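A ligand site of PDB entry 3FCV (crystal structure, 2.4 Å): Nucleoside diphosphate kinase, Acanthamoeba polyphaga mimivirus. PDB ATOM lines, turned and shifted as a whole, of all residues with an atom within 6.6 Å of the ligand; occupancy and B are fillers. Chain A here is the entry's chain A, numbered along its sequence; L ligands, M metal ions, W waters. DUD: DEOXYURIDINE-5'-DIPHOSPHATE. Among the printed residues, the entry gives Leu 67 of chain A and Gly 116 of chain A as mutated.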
ATOM      1  N   LYS A  14      31.445 -13.580 -16.387  1.00  0.00           N
ATOM      2  CA  LYS A  14      30.539 -13.023 -17.393  1.00  0.00           C
ATOM      3  C   LYS A  14      31.254 -12.547 -18.652  1.00  0.00           C
ATOM      4  O   LYS A  14      32.482 -12.395 -18.663  1.00  0.00           O
ATOM      5  CB  LYS A  14      29.713 -11.904 -16.763  1.00  0.00           C
ATOM      6  CG  LYS A  14      28.897 -12.363 -15.557  1.00  0.00           C
ATOM      7  CD  LYS A  14      28.061 -11.248 -14.967  1.00  0.00           C
ATOM      8  CE  LYS A  14      27.241 -11.760 -13.788  1.00  0.00           C
ATOM      9  NZ  LYS A  14      26.357 -10.720 -13.216  1.00  0.00           N
ATOM     10  N   TYR A  55      18.509 -16.796 -13.456  1.00  0.00           N
ATOM     11  CA  TYR A  55      17.948 -15.524 -13.007  1.00  0.00           C
ATOM     12  C   TYR A  55      16.432 -15.538 -12.922  1.00  0.00           C
ATOM     13  O   TYR A  55      15.791 -14.498 -13.111  1.00  0.00           O
ATOM     14  CB  TYR A  55      18.403 -14.380 -13.920  1.00  0.00           C
ATOM     15  CG  TYR A  55      19.849 -13.978 -13.746  1.00  0.00           C
ATOM     16  CD1 TYR A  55      20.744 -14.085 -14.805  1.00  0.00           C
ATOM     17  CD2 TYR A  55      20.318 -13.475 -12.539  1.00  0.00           C
ATOM     18  CE1 TYR A  55      22.076 -13.717 -14.661  1.00  0.00           C
ATOM     19  CE2 TYR A  55      21.648 -13.110 -12.381  1.00  0.00           C
ATOM     20  CZ  TYR A  55      22.514 -13.232 -13.449  1.00  0.00           C
ATOM     21  OH  TYR A  55      23.830 -12.863 -13.308  1.00  0.00           O
ATOM     22  N   GLU A  57      14.547 -15.519 -10.533  1.00  0.00           N
ATOM     23  CA  GLU A  57      14.057 -14.614  -9.499  1.00  0.00           C
ATOM     24  C   GLU A  57      13.867 -13.197 -10.012  1.00  0.00           C
ATOM     25  O   GLU A  57      13.157 -12.393  -9.396  1.00  0.00           O
ATOM     26  CB  GLU A  57      15.014 -14.602  -8.304  1.00  0.00           C
ATOM     27  CG  GLU A  57      15.077 -15.905  -7.520  1.00  0.00           C
ATOM     28  CD  GLU A  57      16.146 -15.893  -6.450  1.00  0.00           C
ATOM     29  OE1 GLU A  57      16.016 -16.655  -5.466  1.00  0.00           O
ATOM     30  OE2 GLU A  57      17.112 -15.111  -6.587  1.00  0.00           O
ATOM     31  N   HIS A  58      14.501 -12.878 -11.136  1.00  0.00           N
ATOM     32  CA  HIS A  58      14.494 -11.514 -11.662  1.00  0.00           C
ATOM     33  C   HIS A  58      13.623 -11.379 -12.904  1.00  0.00           C
ATOM     34  O   HIS A  58      13.769 -10.422 -13.667  1.00  0.00           O
ATOM     35  CB  HIS A  58      15.914 -11.068 -11.991  1.00  0.00           C
ATOM     36  CG  HIS A  58      16.855 -11.138 -10.825  1.00  0.00           C
ATOM     37  ND1 HIS A  58      17.294 -10.014 -10.163  1.00  0.00           N
ATOM     38  CD2 HIS A  58      17.439 -12.196 -10.216  1.00  0.00           C
ATOM     39  CE1 HIS A  58      18.109 -10.376  -9.186  1.00  0.00           C
ATOM     40  NE2 HIS A  58      18.207 -11.695  -9.193  1.00  0.00           N
ATOM     41  N   TYR A  63      14.893  -5.103 -16.096  1.00  0.00           N
ATOM     42  CA  TYR A  63      16.199  -5.311 -16.719  1.00  0.00           C
ATOM     43  C   TYR A  63      16.397  -6.755 -17.159  1.00  0.00           C
ATOM     44  O   TYR A  63      17.393  -7.082 -17.817  1.00  0.00           O
ATOM     45  CB  TYR A  63      17.331  -4.898 -15.774  1.00  0.00           C
ATOM     46  CG  TYR A  63      17.294  -5.576 -14.422  1.00  0.00           C
ATOM     47  CD1 TYR A  63      17.757  -6.875 -14.263  1.00  0.00           C
ATOM     48  CD2 TYR A  63      16.805  -4.922 -13.307  1.00  0.00           C
ATOM     49  CE1 TYR A  63      17.728  -7.503 -13.032  1.00  0.00           C
ATOM     50  CE2 TYR A  63      16.764  -5.531 -12.066  1.00  0.00           C
ATOM     51  CZ  TYR A  63      17.228  -6.819 -11.942  1.00  0.00           C
ATOM     52  OH  TYR A  63      17.193  -7.431 -10.708  1.00  0.00           O
ATOM     53  N   LEU A  67      19.520  -8.124 -19.275  1.00  0.00           N
ATOM     54  CA  LEU A  67      20.387  -9.001 -18.491  1.00  0.00           C
ATOM     55  C   LEU A  67      20.663 -10.300 -19.246  1.00  0.00           C
ATOM     56  O   LEU A  67      21.816 -10.698 -19.417  1.00  0.00           O
ATOM     57  CB  LEU A  67      19.739  -9.313 -17.140  1.00  0.00           C
ATOM     58  CG  LEU A  67      20.426 -10.339 -16.254  1.00  0.00           C
ATOM     59  CD1 LEU A  67      21.817  -9.870 -15.864  1.00  0.00           C
ATOM     60  CD2 LEU A  67      19.584 -10.622 -15.016  1.00  0.00           C
ATOM     61  N   ARG A  91      31.406 -13.816  -1.928  1.00  0.00           N
ATOM     62  CA  ARG A  91      30.492 -12.690  -2.109  1.00  0.00           C
ATOM     63  C   ARG A  91      31.186 -11.385  -1.727  1.00  0.00           C
ATOM     64  O   ARG A  91      31.055 -10.379  -2.410  1.00  0.00           O
ATOM     65  CB  ARG A  91      29.229 -12.880  -1.267  1.00  0.00           C
ATOM     66  CG  ARG A  91      28.245 -13.886  -1.844  1.00  0.00           C
ATOM     67  CD  ARG A  91      27.470 -13.294  -3.000  1.00  0.00           C
ATOM     68  NE  ARG A  91      26.382 -12.434  -2.551  1.00  0.00           N
ATOM     69  CZ  ARG A  91      25.613 -11.711  -3.362  1.00  0.00           C
ATOM     70  NH1 ARG A  91      25.822 -11.738  -4.666  1.00  0.00           N
ATOM     71  NH2 ARG A  91      24.645 -10.960  -2.860  1.00  0.00           N
ATOM     72  N   GLN A  94      33.650 -10.442  -4.240  1.00  0.00           N
ATOM     73  CA  GLN A  94      32.911  -9.977  -5.408  1.00  0.00           C
ATOM     74  C   GLN A  94      32.644  -8.470  -5.359  1.00  0.00           C
ATOM     75  O   GLN A  94      32.975  -7.744  -6.296  1.00  0.00           O
ATOM     76  CB  GLN A  94      31.602 -10.745  -5.536  1.00  0.00           C
ATOM     77  CG  GLN A  94      30.719 -10.306  -6.695  1.00  0.00           C
ATOM     78  CD  GLN A  94      29.344 -10.930  -6.651  1.00  0.00           C
ATOM     79  OE1 GLN A  94      28.771 -11.303  -7.675  1.00  0.00           O
ATOM     80  NE2 GLN A  94      28.796 -11.073  -5.435  1.00  0.00           N
ATOM     81  N   GLY A  95      32.054  -8.019  -4.263  1.00  0.00           N
ATOM     82  CA  GLY A  95      31.715  -6.612  -4.109  1.00  0.00           C
ATOM     83  C   GLY A  95      30.268  -6.336  -4.472  1.00  0.00           C
ATOM     84  O   GLY A  95      29.634  -7.134  -5.163  1.00  0.00           O
ATOM     85  N   ASN A  96      29.761  -5.192  -4.031  1.00  0.00           N
ATOM     86  CA  ASN A  96      28.374  -4.819  -4.281  1.00  0.00           C
ATOM     87  C   ASN A  96      28.035  -4.746  -5.769  1.00  0.00           C
ATOM     88  O   ASN A  96      28.910  -4.528  -6.608  1.00  0.00           O
ATOM     89  CB  ASN A  96      28.059  -3.471  -3.619  1.00  0.00           C
ATOM     90  CG  ASN A  96      26.580  -3.169  -3.586  1.00  0.00           C
ATOM     91  OD1 ASN A  96      26.095  -2.290  -4.300  1.00  0.00           O
ATOM     92  ND2 ASN A  96      25.840  -3.899  -2.760  1.00  0.00           N
ATOM     93  N   THR A  97      26.758  -4.934  -6.099  1.00  0.00           N
ATOM     94  CA  THR A  97      26.285  -4.878  -7.477  1.00  0.00           C
ATOM     95  C   THR A  97      26.442  -3.463  -8.018  1.00  0.00           C
ATOM     96  O   THR A  97      26.728  -3.266  -9.200  1.00  0.00           O
ATOM     97  CB  THR A  97      24.803  -5.277  -7.584  1.00  0.00           C
ATOM     98  OG1 THR A  97      24.504  -6.322  -6.656  1.00  0.00           O
ATOM     99  CG2 THR A  97      24.469  -5.741  -8.999  1.00  0.00           C
ATOM    100  N   ASN A  98      26.249  -2.491  -7.138  1.00  0.00           N
ATOM    101  CA  ASN A  98      26.259  -1.086  -7.526  1.00  0.00           C
ATOM    102  C   ASN A  98      27.664  -0.480  -7.546  1.00  0.00           C
ATOM    103  O   ASN A  98      28.416  -0.622  -6.579  1.00  0.00           O
ATOM    104  CB  ASN A  98      25.349  -0.283  -6.604  1.00  0.00           C
ATOM    105  CG  ASN A  98      24.880   1.019  -7.227  1.00  0.00           C
ATOM    106  OD1 ASN A  98      25.687   1.806  -7.733  1.00  0.00           O
ATOM    107  ND2 ASN A  98      23.576   1.246  -7.204  1.00  0.00           N
ATOM    108  N   ARG A 108      34.467  -6.153  -8.190  1.00  0.00           N
ATOM    109  CA  ARG A 108      33.628  -5.126  -8.797  1.00  0.00           C
ATOM    110  C   ARG A 108      34.118  -3.728  -8.428  1.00  0.00           C
ATOM    111  O   ARG A 108      34.127  -2.814  -9.258  1.00  0.00           O
ATOM    112  CB  ARG A 108      32.170  -5.303  -8.381  1.00  0.00           C
ATOM    113  CG  ARG A 108      31.498  -6.530  -8.957  1.00  0.00           C
ATOM    114  CD  ARG A 108      30.120  -6.754  -8.358  1.00  0.00           C
ATOM    115  NE  ARG A 108      29.353  -7.742  -9.109  1.00  0.00           N
ATOM    116  CZ  ARG A 108      28.169  -8.214  -8.730  1.00  0.00           C
ATOM    117  NH1 ARG A 108      27.629  -7.802  -7.595  1.00  0.00           N
ATOM    118  NH2 ARG A 108      27.542  -9.100  -9.482  1.00  0.00           N
ATOM    119  N   ASP A 114      29.777  -0.672 -14.092  1.00  0.00           N
ATOM    120  CA  ASP A 114      28.374  -0.678 -14.483  1.00  0.00           C
ATOM    121  C   ASP A 114      27.621  -1.655 -13.594  1.00  0.00           C
ATOM    122  O   ASP A 114      28.198  -2.624 -13.109  1.00  0.00           O
ATOM    123  CB  ASP A 114      28.241  -1.092 -15.951  1.00  0.00           C
ATOM    124  CG  ASP A 114      26.818  -0.989 -16.456  1.00  0.00           C
ATOM    125  OD1 ASP A 114      26.231  -2.035 -16.807  1.00  0.00           O
ATOM    126  OD2 ASP A 114      26.279   0.145 -16.502  1.00  0.00           O
ATOM    127  N   ILE A 115      26.336  -1.394 -13.383  1.00  0.00           N
ATOM    128  CA  ILE A 115      25.534  -2.261 -12.518  1.00  0.00           C
ATOM    129  C   ILE A 115      25.077  -3.507 -13.268  1.00  0.00           C
ATOM    130  O   ILE A 115      24.779  -4.532 -12.652  1.00  0.00           O
ATOM    131  CB  ILE A 115      24.304  -1.523 -11.938  1.00  0.00           C
ATOM    132  CG1 ILE A 115      23.708  -2.326 -10.776  1.00  0.00           C
ATOM    133  CG2 ILE A 115      23.263  -1.276 -13.029  1.00  0.00           C
ATOM    134  CD1 ILE A 115      22.637  -1.592 -10.011  1.00  0.00           C
ATOM    135  N   GLY A 116      25.036  -3.431 -14.592  1.00  0.00           N
ATOM    136  CA  GLY A 116      24.681  -4.571 -15.418  1.00  0.00           C
ATOM    137  C   GLY A 116      25.897  -5.418 -15.736  1.00  0.00           C
ATOM    138  O   GLY A 116      25.934  -6.604 -15.440  1.00  0.00           O
ATOM    139  N   GLU A 117      26.893  -4.785 -16.354  1.00  0.00           N
ATOM    140  CA  GLU A 117      28.141  -5.463 -16.667  1.00  0.00           C
ATOM    141  C   GLU A 117      29.067  -5.434 -15.453  1.00  0.00           C
ATOM    142  O   GLU A 117      29.893  -4.518 -15.310  1.00  0.00           O
ATOM    143  CB  GLU A 117      28.810  -4.811 -17.884  1.00  0.00           C
ATOM    144  CG  GLU A 117      27.961  -4.893 -19.145  1.00  0.00           C
ATOM    145  CD  GLU A 117      28.526  -4.083 -20.298  1.00  0.00           C
ATOM    146  OE1 GLU A 117      28.148  -4.348 -21.452  1.00  0.00           O
ATOM    147  OE2 GLU A 117      29.346  -3.180 -20.034  1.00  0.00           O
ATOM    148  N   ASN A 118      28.929  -6.434 -14.587  1.00  0.00           N
ATOM    149  CA  ASN A 118      29.668  -6.462 -13.334  1.00  0.00           C
ATOM    150  C   ASN A 118      30.611  -7.657 -13.198  1.00  0.00           C
ATOM    151  O   ASN A 118      30.963  -8.060 -12.086  1.00  0.00           O
ATOM    152  CB  ASN A 118      28.705  -6.403 -12.144  1.00  0.00           C
ATOM    153  CG  ASN A 118      27.595  -7.422 -12.240  1.00  0.00           C
ATOM    154  OD1 ASN A 118      27.831  -8.597 -12.499  1.00  0.00           O
ATOM    155  ND2 ASN A 118      26.355  -6.972 -12.032  1.00  0.00           N
ATOM    156  N   ILE A 120      31.240 -10.619 -12.626  1.00  0.00           N
ATOM    157  CA  ILE A 120      31.160 -11.876 -11.890  1.00  0.00           C
ATOM    158  C   ILE A 120      29.826 -12.108 -11.181  1.00  0.00           C
ATOM    159  O   ILE A 120      29.244 -11.185 -10.618  1.00  0.00           O
ATOM    160  CB  ILE A 120      32.301 -11.971 -10.851  1.00  0.00           C
ATOM    161  CG1 ILE A 120      32.186 -13.284 -10.067  1.00  0.00           C
ATOM    162  CG2 ILE A 120      32.272 -10.781  -9.908  1.00  0.00           C
ATOM    163  CD1 ILE A 120      33.385 -13.566  -9.173  1.00  0.00           C
ATOM    164  N   HIS A 121      29.365 -13.345 -11.224  1.00  0.00           N
ATOM    165  CA  HIS A 121      28.257 -13.788 -10.397  1.00  0.00           C
ATOM    166  C   HIS A 121      28.757 -14.722  -9.308  1.00  0.00           C
ATOM    167  O   HIS A 121      29.743 -15.433  -9.489  1.00  0.00           O
ATOM    168  CB  HIS A 121      27.183 -14.506 -11.225  1.00  0.00           C
ATOM    169  CG  HIS A 121      26.209 -15.274 -10.388  1.00  0.00           C
ATOM    170  ND1 HIS A 121      25.009 -14.737  -9.962  1.00  0.00           N
ATOM    171  CD2 HIS A 121      26.263 -16.532  -9.890  1.00  0.00           C
ATOM    172  CE1 HIS A 121      24.367 -15.636  -9.234  1.00  0.00           C
ATOM    173  NE2 HIS A 121      25.106 -16.729  -9.176  1.00  0.00           N
ATOM    174  N   ALA A 122      28.077 -14.715  -8.161  1.00  0.00           N
ATOM    175  CA  ALA A 122      28.407 -15.614  -7.069  1.00  0.00           C
ATOM    176  C   ALA A 122      27.152 -15.913  -6.263  1.00  0.00           C
ATOM    177  O   ALA A 122      26.441 -14.992  -5.866  1.00  0.00           O
ATOM    178  CB  ALA A 122      29.483 -15.020  -6.186  1.00  0.00           C
ATOM    179  N   ASP A 124      24.491 -16.401  -3.488  1.00  0.00           N
ATOM    180  CA  ASP A 124      24.371 -15.552  -2.310  1.00  0.00           C
ATOM    181  C   ASP A 124      23.998 -16.314  -1.036  1.00  0.00           C
ATOM    182  O   ASP A 124      23.992 -15.752   0.053  1.00  0.00           O
ATOM    183  CB  ASP A 124      23.365 -14.423  -2.561  1.00  0.00           C
ATOM    184  CG  ASP A 124      21.973 -14.934  -2.872  1.00  0.00           C
ATOM    185  OD1 ASP A 124      21.654 -16.081  -2.484  1.00  0.00           O
ATOM    186  OD2 ASP A 124      21.195 -14.191  -3.504  1.00  0.00           O
HETATM  187  N1  DUD L   1      20.988  -5.980 -12.379  1.00  0.00           N
HETATM  188  C2  DUD L   1      20.725  -4.836 -13.170  1.00  0.00           C
HETATM  189  N3  DUD L   1      20.120  -3.771 -12.633  1.00  0.00           N
HETATM  190  C4  DUD L   1      19.759  -3.769 -11.343  1.00  0.00           C
HETATM  191  C5  DUD L   1      20.011  -4.880 -10.546  1.00  0.00           C
HETATM  192  C6  DUD L   1      20.646  -5.989 -11.094  1.00  0.00           C
HETATM  193  O2  DUD L   1      21.059  -4.823 -14.374  1.00  0.00           O
HETATM  194  O4  DUD L   1      19.194  -2.769 -10.855  1.00  0.00           O
HETATM  195  C1' DUD L   1      21.649  -7.160 -12.929  1.00  0.00           C
HETATM  196  C2' DUD L   1      23.093  -7.236 -12.429  1.00  0.00           C
HETATM  197  C3' DUD L   1      23.126  -8.490 -11.574  1.00  0.00           C
HETATM  198  C4' DUD L   1      21.880  -9.269 -11.949  1.00  0.00           C
HETATM  199  O4' DUD L   1      20.957  -8.300 -12.437  1.00  0.00           O
HETATM  200  O3' DUD L   1      24.323  -9.233 -11.852  1.00  0.00           O
HETATM  201  C5' DUD L   1      21.270  -9.984 -10.748  1.00  0.00           C
HETATM  202  O5' DUD L   1      21.074  -8.988  -9.747  1.00  0.00           O
HETATM  203  PA  DUD L   1      21.544  -9.261  -8.230  1.00  0.00           P
HETATM  204  O1A DUD L   1      21.435 -10.744  -7.960  1.00  0.00           O
HETATM  205  O2A DUD L   1      20.836  -8.276  -7.326  1.00  0.00           O
HETATM  206  O3A DUD L   1      23.100  -8.836  -8.346  1.00  0.00           O
HETATM  207  PB  DUD L   1      24.283  -9.688  -7.678  1.00  0.00           P
HETATM  208  O1B DUD L   1      23.607 -10.680  -6.763  1.00  0.00           O
HETATM  209  O2B DUD L   1      25.127  -8.670  -6.951  1.00  0.00           O
HETATM  210  O3B DUD L   1      24.966 -10.301  -8.878  1.00  0.00           O
HETATM  211 MG    MG M   1      21.629 -12.762  -6.070  1.00  0.00          MG
HETATM  212  O   HOH W   1      26.106 -12.633  -7.506  1.00  0.00           O
HETATM  213  O   HOH W   2      25.040 -12.015 -10.916  1.00  0.00           O
HETATM  214  O   HOH W   3      21.658  -6.262  -5.274  1.00  0.00           O
HETATM  215  O   HOH W   4      21.328  -6.180 -16.512  1.00  0.00           O
HETATM  216  O   HOH W   5      25.405  -7.762  -4.342  1.00  0.00           O
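OG1 of Thr 97 lies within hydrogen-bond range of O2B of the ligand (2.4 Å).
The guanidinium group (NH1) of Arg 108 lies within salt-bridge range of an oxygen (O2B) of the ligand (2.7 Å).
The side-chain amino group (NZ) of Lys 14 sits at hydrogen-bond distance from an oxygen (O3') of the ligand.
O3' of the ligand is in hydrogen-bond range of ND2 of Asn 118 (3.0 Å).
O1B of the ligand lies within salt-bridge range of NH1 of Arg 91, at 3.2 Å.
Merely in contact with the ligand: Tyr 55 (3.5 Å), His 58 (3.3 Å), Tyr 63 (3.4 Å), Leu 67 (3.7 Å), Ile 115 (3.2 Å) and Gly 116 (3.8 Å).
Hydrophobic or aromatic side chains within 4 Å of the ligand: Tyr 55, His 58, Tyr 63, Leu 67 and Ile 115.
11 residues have an atom within 4 Å of the ligand: Lys 14, Tyr 55, His 58, Tyr 63, Leu 67, Arg 91, Thr 97, Arg 108, Ile 115, Gly 116 and Asn 118.
The nearest printed residue that does not touch the ligand is Gln 94 (4.1 Å).
The guanidinium group of Arg 108 is in hydrogen-bond range of the side-chain amide oxygen of Asn 118.
The backbone carbonyl oxygen (O) of Gln 94 is in hydrogen-bond range of the backbone NH (N) of Arg 108 (2.9 Å).
The backbone carbonyl oxygen of Ile 120 is in hydrogen-bond range of the guanidinium group of Arg 108, at 2.9 Å.
NH1 of Arg 108 sits at hydrogen-bond distance from O of Gly 95.
OD1 of Asn 118 is in hydrogen-bond range of NZ of Lys 14.
The backbone carbonyl oxygen (O) of Ile 120 sits close to the side-chain amide oxygen (OD1) of Asn 118, 3.5 Å away.
NH1 of Arg 91 lies close to NE2 of Gln 94, 3.1 Å away.
The backbone NH (N) of Gly 116 sits at hydrogen-bond distance from the side-chain carboxylate (OD1) of Asp 114 (2.9 Å).
Water W2 lies within hydrogen-bond range of O3B of the ligand (2.7 Å), OH of Tyr 55 (2.8 Å), ND1 of His 121 (2.9 Å) and NZ of Lys 14 (2.9 Å).
Water W5 lies within hydrogen-bond range of O2B of the ligand (2.8 Å) and OG1 of Thr 97 (2.9 Å).
Water W1 lies within hydrogen-bond range of O of Ala 122 (2.9 Å), O3B of the ligand (2.9 Å), OE1 of Gln 94 (3.0 Å), NH1 of Arg 91 (3.0 Å) and ND1 of His 121 (3.4 Å).
Water W3 lies within hydrogen-bond range of O2A of the ligand and OG1 of Thr 97.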
